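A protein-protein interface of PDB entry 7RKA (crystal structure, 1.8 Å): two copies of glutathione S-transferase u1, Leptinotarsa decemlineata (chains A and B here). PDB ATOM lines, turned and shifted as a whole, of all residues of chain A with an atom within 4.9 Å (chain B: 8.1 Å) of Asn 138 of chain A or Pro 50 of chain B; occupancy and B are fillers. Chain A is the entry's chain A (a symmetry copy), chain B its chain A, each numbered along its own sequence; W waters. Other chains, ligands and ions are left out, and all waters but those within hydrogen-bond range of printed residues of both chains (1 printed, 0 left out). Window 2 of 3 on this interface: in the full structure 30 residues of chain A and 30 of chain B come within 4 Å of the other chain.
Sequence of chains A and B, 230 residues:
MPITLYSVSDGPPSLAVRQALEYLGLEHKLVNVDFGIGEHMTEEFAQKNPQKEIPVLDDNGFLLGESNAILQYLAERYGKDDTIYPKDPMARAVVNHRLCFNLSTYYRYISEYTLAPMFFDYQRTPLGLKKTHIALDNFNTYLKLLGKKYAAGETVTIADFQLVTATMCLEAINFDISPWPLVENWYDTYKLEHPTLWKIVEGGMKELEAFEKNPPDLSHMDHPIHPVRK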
ATOM      1  N   PHE A 101      25.683  17.186  15.510  1.00  0.00           N
ATOM      2  CA  PHE A 101      25.076  18.506  15.394  1.00  0.00           C
ATOM      3  C   PHE A 101      25.576  19.422  16.504  1.00  0.00           C
ATOM      4  O   PHE A 101      25.888  20.603  16.270  1.00  0.00           O
ATOM      5  CB  PHE A 101      23.545  18.352  15.421  1.00  0.00           C
ATOM      6  CG  PHE A 101      22.783  19.652  15.583  1.00  0.00           C
ATOM      7  CD1 PHE A 101      22.805  20.631  14.591  1.00  0.00           C
ATOM      8  CD2 PHE A 101      22.026  19.883  16.732  1.00  0.00           C
ATOM      9  CE1 PHE A 101      22.123  21.848  14.774  1.00  0.00           C
ATOM     10  CE2 PHE A 101      21.326  21.077  16.900  1.00  0.00           C
ATOM     11  CZ  PHE A 101      21.389  22.061  15.919  1.00  0.00           C
ATOM     12  N   THR A 105      27.860  22.456  15.013  1.00  0.00           N
ATOM     13  CA  THR A 105      26.943  23.545  14.714  1.00  0.00           C
ATOM     14  C   THR A 105      26.415  24.214  15.985  1.00  0.00           C
ATOM     15  O   THR A 105      26.682  25.399  16.214  1.00  0.00           O
ATOM     16  CB  THR A 105      25.775  23.049  13.856  1.00  0.00           C
ATOM     17  OG1 THR A 105      26.267  22.498  12.629  1.00  0.00           O
ATOM     18  CG2 THR A 105      24.834  24.213  13.524  1.00  0.00           C
ATOM     19  N   ILE A 134      20.630  30.670  13.771  1.00  0.00           N
ATOM     20  CA  ILE A 134      20.471  29.547  12.852  1.00  0.00           C
ATOM     21  C   ILE A 134      20.574  28.226  13.612  1.00  0.00           C
ATOM     22  O   ILE A 134      19.802  27.284  13.365  1.00  0.00           O
ATOM     23  CB  ILE A 134      21.522  29.629  11.728  1.00  0.00           C
ATOM     24  CG1 ILE A 134      21.236  30.816  10.796  1.00  0.00           C
ATOM     25  CG2 ILE A 134      21.566  28.333  10.934  1.00  0.00           C
ATOM     26  CD1 ILE A 134      22.376  31.098   9.841  1.00  0.00           C
ATOM     27  N   ALA A 135      21.538  28.135  14.535  1.00  0.00           N
ATOM     28  CA  ALA A 135      21.704  26.921  15.337  1.00  0.00           C
ATOM     29  C   ALA A 135      20.448  26.622  16.145  1.00  0.00           C
ATOM     30  O   ALA A 135      19.996  25.470  16.207  1.00  0.00           O
ATOM     31  CB  ALA A 135      22.918  27.064  16.257  1.00  0.00           C
ATOM     32  N   LEU A 136      19.853  27.658  16.745  1.00  0.00           N
ATOM     33  CA  LEU A 136      18.620  27.471  17.500  1.00  0.00           C
ATOM     34  C   LEU A 136      17.448  27.132  16.582  1.00  0.00           C
ATOM     35  O   LEU A 136      16.646  26.250  16.906  1.00  0.00           O
ATOM     36  CB  LEU A 136      18.316  28.723  18.320  1.00  0.00           C
ATOM     37  CG  LEU A 136      19.221  28.948  19.551  1.00  0.00           C
ATOM     38  CD1 LEU A 136      19.315  30.437  19.839  1.00  0.00           C
ATOM     39  CD2 LEU A 136      18.681  28.182  20.752  1.00  0.00           C
ATOM     40  N   ASP A 137      17.338  27.805  15.429  1.00  0.00           N
ATOM     41  CA  ASP A 137      16.351  27.388  14.423  1.00  0.00           C
ATOM     42  C   ASP A 137      16.472  25.894  14.120  1.00  0.00           C
ATOM     43  O   ASP A 137      15.474  25.161  14.109  1.00  0.00           O
ATOM     44  CB  ASP A 137      16.525  28.167  13.115  1.00  0.00           C
ATOM     45  CG  ASP A 137      16.072  29.645  13.201  1.00  0.00           C
ATOM     46  OD1 ASP A 137      15.345  30.070  14.121  1.00  0.00           O
ATOM     47  OD2 ASP A 137      16.484  30.387  12.303  1.00  0.00           O
ATOM     48  N   ASN A 138      17.696  25.440  13.818  1.00  0.00           N
ATOM     49  CA  ASN A 138      17.923  24.038  13.468  1.00  0.00           C
ATOM     50  C   ASN A 138      17.478  23.101  14.587  1.00  0.00           C
ATOM     51  O   ASN A 138      16.854  22.054  14.334  1.00  0.00           O
ATOM     52  CB  ASN A 138      19.407  23.786  13.181  1.00  0.00           C
ATOM     53  CG  ASN A 138      19.927  24.503  11.953  1.00  0.00           C
ATOM     54  OD1 ASN A 138      19.179  25.002  11.094  1.00  0.00           O
ATOM     55  ND2 ASN A 138      21.236  24.576  11.880  1.00  0.00           N
ATOM     56  N   PHE A 139      17.817  23.431  15.840  1.00  0.00           N
ATOM     57  CA  PHE A 139      17.466  22.552  16.954  1.00  0.00           C
ATOM     58  C   PHE A 139      15.950  22.524  17.166  1.00  0.00           C
ATOM     59  O   PHE A 139      15.359  21.459  17.397  1.00  0.00           O
ATOM     60  CB  PHE A 139      18.226  23.022  18.211  1.00  0.00           C
ATOM     61  CG  PHE A 139      18.108  22.119  19.422  1.00  0.00           C
ATOM     62  CD1 PHE A 139      17.803  20.761  19.313  1.00  0.00           C
ATOM     63  CD2 PHE A 139      18.335  22.651  20.695  1.00  0.00           C
ATOM     64  CE1 PHE A 139      17.703  19.958  20.423  1.00  0.00           C
ATOM     65  CE2 PHE A 139      18.238  21.836  21.825  1.00  0.00           C
ATOM     66  CZ  PHE A 139      17.940  20.489  21.686  1.00  0.00           C
ATOM     67  N   ASN A 140      15.301  23.682  17.080  1.00  0.00           N
ATOM     68  CA  ASN A 140      13.846  23.729  17.167  1.00  0.00           C
ATOM     69  C   ASN A 140      13.217  22.861  16.092  1.00  0.00           C
ATOM     70  O   ASN A 140      12.286  22.090  16.366  1.00  0.00           O
ATOM     71  CB  ASN A 140      13.382  25.193  17.035  1.00  0.00           C
ATOM     72  CG  ASN A 140      11.986  25.442  17.607  1.00  0.00           C
ATOM     73  OD1 ASN A 140      11.806  25.603  18.819  1.00  0.00           O
ATOM     74  ND2 ASN A 140      10.999  25.506  16.724  1.00  0.00           N
ATOM     75  N   THR A 141      13.747  22.936  14.868  1.00  0.00           N
ATOM     76  CA  THR A 141      13.228  22.108  13.781  1.00  0.00           C
ATOM     77  C   THR A 141      13.468  20.625  14.037  1.00  0.00           C
ATOM     78  O   THR A 141      12.575  19.801  13.807  1.00  0.00           O
ATOM     79  CB  THR A 141      13.851  22.533  12.449  1.00  0.00           C
ATOM     80  OG1 THR A 141      13.463  23.874  12.125  1.00  0.00           O
ATOM     81  CG2 THR A 141      13.407  21.602  11.301  1.00  0.00           C
ATOM     82  N   TYR A 142      14.652  20.259  14.556  1.00  0.00           N
ATOM     83  CA  TYR A 142      14.919  18.851  14.846  1.00  0.00           C
ATOM     84  C   TYR A 142      13.967  18.300  15.897  1.00  0.00           C
ATOM     85  O   TYR A 142      13.491  17.161  15.788  1.00  0.00           O
ATOM     86  CB  TYR A 142      16.364  18.651  15.326  1.00  0.00           C
ATOM     87  CG  TYR A 142      17.379  18.626  14.218  1.00  0.00           C
ATOM     88  CD1 TYR A 142      17.194  17.832  13.091  1.00  0.00           C
ATOM     89  CD2 TYR A 142      18.525  19.413  14.292  1.00  0.00           C
ATOM     90  CE1 TYR A 142      18.122  17.822  12.068  1.00  0.00           C
ATOM     91  CE2 TYR A 142      19.454  19.412  13.274  1.00  0.00           C
ATOM     92  CZ  TYR A 142      19.254  18.606  12.166  1.00  0.00           C
ATOM     93  OH  TYR A 142      20.201  18.590  11.154  1.00  0.00           O
ATOM     94  N   LEU A 145      10.711  17.756  14.102  1.00  0.00           N
ATOM     95  CA  LEU A 145      10.768  16.671  13.123  1.00  0.00           C
ATOM     96  C   LEU A 145      10.701  15.308  13.796  1.00  0.00           C
ATOM     97  O   LEU A 145       9.914  14.444  13.395  1.00  0.00           O
ATOM     98  CB  LEU A 145      12.045  16.773  12.295  1.00  0.00           C
ATOM     99  CG  LEU A 145      12.074  17.764  11.144  1.00  0.00           C
ATOM    100  CD1 LEU A 145      13.533  18.046  10.754  1.00  0.00           C
ATOM    101  CD2 LEU A 145      11.301  17.227   9.953  1.00  0.00           C
ATOM    102  N   PHE B  45      12.651  16.795   0.338  1.00  0.00           N
ATOM    103  CA  PHE B  45      12.889  16.660   1.771  1.00  0.00           C
ATOM    104  C   PHE B  45      13.747  17.796   2.323  1.00  0.00           C
ATOM    105  O   PHE B  45      14.615  17.569   3.171  1.00  0.00           O
ATOM    106  CB  PHE B  45      13.516  15.282   2.071  1.00  0.00           C
ATOM    107  CG  PHE B  45      14.943  15.127   1.582  1.00  0.00           C
ATOM    108  CD1 PHE B  45      15.995  15.082   2.471  1.00  0.00           C
ATOM    109  CD2 PHE B  45      15.223  15.000   0.235  1.00  0.00           C
ATOM    110  CE1 PHE B  45      17.297  14.940   2.023  1.00  0.00           C
ATOM    111  CE2 PHE B  45      16.525  14.858  -0.212  1.00  0.00           C
ATOM    112  CZ  PHE B  45      17.562  14.838   0.682  1.00  0.00           C
ATOM    113  N   ALA B  46      13.458  19.037   1.905  1.00  0.00           N
ATOM    114  CA  ALA B  46      14.206  20.189   2.410  1.00  0.00           C
ATOM    115  C   ALA B  46      13.684  20.687   3.760  1.00  0.00           C
ATOM    116  O   ALA B  46      14.473  21.162   4.585  1.00  0.00           O
ATOM    117  CB  ALA B  46      14.171  21.333   1.393  1.00  0.00           C
ATOM    118  N   GLN B  47      12.372  20.608   4.002  1.00  0.00           N
ATOM    119  CA  GLN B  47      11.822  20.896   5.325  1.00  0.00           C
ATOM    120  C   GLN B  47      12.358  19.933   6.378  1.00  0.00           C
ATOM    121  O   GLN B  47      12.325  20.250   7.578  1.00  0.00           O
ATOM    122  CB  GLN B  47      10.295  20.827   5.225  1.00  0.00           C
ATOM    123  CG  GLN B  47       9.460  21.226   6.473  1.00  0.00           C
ATOM    124  CD  GLN B  47       9.017  22.691   6.421  1.00  0.00           C
ATOM    125  OE1 GLN B  47       8.112  23.047   5.659  1.00  0.00           O
ATOM    126  NE2 GLN B  47       9.611  23.531   7.271  1.00  0.00           N
ATOM    127  N   LYS B  48      12.904  18.788   5.934  1.00  0.00           N
ATOM    128  CA  LYS B  48      13.337  17.694   6.801  1.00  0.00           C
ATOM    129  C   LYS B  48      14.801  17.826   7.185  1.00  0.00           C
ATOM    130  O   LYS B  48      15.233  17.198   8.157  1.00  0.00           O
ATOM    131  CB  LYS B  48      13.152  16.332   6.094  1.00  0.00           C
ATOM    132  CG  LYS B  48      11.636  15.769   6.073  1.00  0.00           C
ATOM    133  CD  LYS B  48      11.020  16.793   5.109  1.00  0.00           C
ATOM    134  CE  LYS B  48       9.543  16.567   4.749  1.00  0.00           C
ATOM    135  NZ  LYS B  48       9.581  17.867   3.875  1.00  0.00           N
ATOM    136  N   ASN B  49      15.575  18.595   6.412  1.00  0.00           N
ATOM    137  CA  ASN B  49      16.968  18.912   6.715  1.00  0.00           C
ATOM    138  C   ASN B  49      17.099  20.411   6.940  1.00  0.00           C
ATOM    139  O   ASN B  49      17.464  21.161   6.017  1.00  0.00           O
ATOM    140  CB  ASN B  49      17.912  18.457   5.601  1.00  0.00           C
ATOM    141  CG  ASN B  49      17.928  16.974   5.441  1.00  0.00           C
ATOM    142  OD1 ASN B  49      17.706  16.227   6.399  1.00  0.00           O
ATOM    143  ND2 ASN B  49      18.244  16.522   4.238  1.00  0.00           N
ATOM    144  N   PRO B  50      16.831  20.898   8.149  1.00  0.00           N
ATOM    145  CA  PRO B  50      16.922  22.351   8.387  1.00  0.00           C
ATOM    146  C   PRO B  50      18.295  22.923   8.093  1.00  0.00           C
ATOM    147  O   PRO B  50      18.395  24.063   7.619  1.00  0.00           O
ATOM    148  CB  PRO B  50      16.555  22.493   9.872  1.00  0.00           C
ATOM    149  CG  PRO B  50      16.796  21.088  10.478  1.00  0.00           C
ATOM    150  CD  PRO B  50      16.456  20.130   9.353  1.00  0.00           C
ATOM    151  N   GLN B  51      19.362  22.172   8.350  1.00  0.00           N
ATOM    152  CA  GLN B  51      20.707  22.696   8.135  1.00  0.00           C
ATOM    153  C   GLN B  51      21.061  22.836   6.663  1.00  0.00           C
ATOM    154  O   GLN B  51      22.200  23.212   6.367  1.00  0.00           O
ATOM    155  CB  GLN B  51      21.745  21.788   8.801  1.00  0.00           C
ATOM    156  CG  GLN B  51      21.817  21.908  10.314  1.00  0.00           C
ATOM    157  CD  GLN B  51      22.849  20.987  10.918  1.00  0.00           C
ATOM    158  OE1 GLN B  51      22.510  19.913  11.416  1.00  0.00           O
ATOM    159  NE2 GLN B  51      24.124  21.388  10.860  1.00  0.00           N
ATOM    160  N   LYS B  52      20.135  22.564   5.743  1.00  0.00           N
ATOM    161  CA  LYS B  52      20.476  22.372   4.335  1.00  0.00           C
ATOM    162  C   LYS B  52      21.579  21.320   4.253  1.00  0.00           C
ATOM    163  O   LYS B  52      22.687  21.554   3.770  1.00  0.00           O
ATOM    164  CB  LYS B  52      20.885  23.695   3.679  1.00  0.00           C
ATOM    165  CG  LYS B  52      19.973  24.870   4.043  1.00  0.00           C
ATOM    166  CD  LYS B  52      18.494  24.540   3.816  1.00  0.00           C
ATOM    167  CE  LYS B  52      17.600  25.749   4.102  1.00  0.00           C
ATOM    168  NZ  LYS B  52      17.663  26.167   5.541  1.00  0.00           N
ATOM    169  N   GLU B  53      21.246  20.146   4.785  1.00  0.00           N
ATOM    170  CA  GLU B  53      22.228  19.173   5.247  1.00  0.00           C
ATOM    171  C   GLU B  53      22.635  18.279   4.084  1.00  0.00           C
ATOM    172  O   GLU B  53      21.790  17.576   3.519  1.00  0.00           O
ATOM    173  CB  GLU B  53      21.619  18.367   6.399  1.00  0.00           C
ATOM    174  CG  GLU B  53      22.587  17.822   7.431  1.00  0.00           C
ATOM    175  CD  GLU B  53      21.862  17.202   8.637  1.00  0.00           C
ATOM    176  OE1 GLU B  53      20.614  17.054   8.626  1.00  0.00           O
ATOM    177  OE2 GLU B  53      22.542  16.887   9.615  1.00  0.00           O
HETATM  178  O   HOH W   1      19.483  19.212   8.535  1.00  0.00           O
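Water W1 lies within hydrogen-bond range of the side-chain carboxylate of Glu 53 of chain B (2.4 Å), the side-chain hydroxyl of Tyr 142 of chain A (2.8 Å) and the backbone NH of Gln 51 of chain B (3.0 Å).
The backbone carbonyl oxygen (O) of Asp 137 of chain A is in hydrogen-bond range of the side-chain hydroxyl (OG1) of Thr 141 of chain A, 3.1 Å away.
O of Ile 134 of chain A sits close to OD1 of Asn 138 of chain A.
O of Pro 50 of chain B lies within hydrogen-bond range of NZ of Lys 52 of chain B (3.0 Å).
Of the 12 printed residues of chain A, 6 touch a printed residue of chain B.
Hydrophobic or aromatic side chains of chain A that line the printed part of chain B: Phe 101, Tyr 142 and Leu 145.
Among the printed residues, no Asp or Glu carboxylate lies within 4 Å of a Lys or Arg side-chain nitrogen of the other chain.
CD1 of Phe 101 of chain A touches OE1 of Gln 51 of chain B, 3.3 Å away.
OD1 of Asn 138 of chain A touches O of Pro 50 of chain B, at 3.7 Å.
Asn 138 of chain A touches Gln 51 of chain B (ND2 to CG, 3.1 Å).
CG of Pro 50 of chain B touches CG2 of Thr 141 of chain A, at 3.5 Å.
Tyr 142 of chain A touches Pro 50 of chain B (CE1 to CG, 3.9 Å).
Leu 145 of chain A touches Gln 47 of chain B.
Leu 145 of chain A touches Lys 48 of chain B.
Pro 50 of chain B touches Leu 145 of chain A.
No position is printed for both chains.
Of the 11 pairs that touch across the chains among the printed residues, none has its exchanged pair printed and touching as well.
The side-chain carboxylate (OE1) of Glu 53 of chain B is in hydrogen-bond range of the side-chain hydroxyl (OH) of Tyr 142 of chain A (3.0 Å).
OE1 of Gln 51 of chain B sits at hydrogen-bond distance from OH of Tyr 142 of chain A (2.7 Å).
NE2 of Gln 51 of chain B sits at hydrogen-bond distance from OG1 of Thr 105 of chain A, at 3.0 Å.
Printed residues of chain B within 4 Å of Thr 141 of chain A: Pro 50 (3.5 Å).
Of the printed residues of chain B, Leu 145 of chain A touches Gln 47 (3.98 Å), Lys 48 (3.2 Å) and Pro 50 (3.9 Å).
Of the printed residues of chain A, Gln 47 of chain B touches Leu 145.
Of the printed residues of chain A, Lys 48 of chain B touches Leu 145.
Pro 50 of chain B touches four residues of chain A.
Printed residues of chain A within 4 Å of Gln 51 of chain B: Phe 101 (3.3 Å), Thr 105 (3.0 Å), Asn 138 (3.1 Å) and Tyr 142 (2.7 Å).
The nearest residue of chain B that does not touch Asn 138 of chain A is Lys 52 of chain B (5.9 Å).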
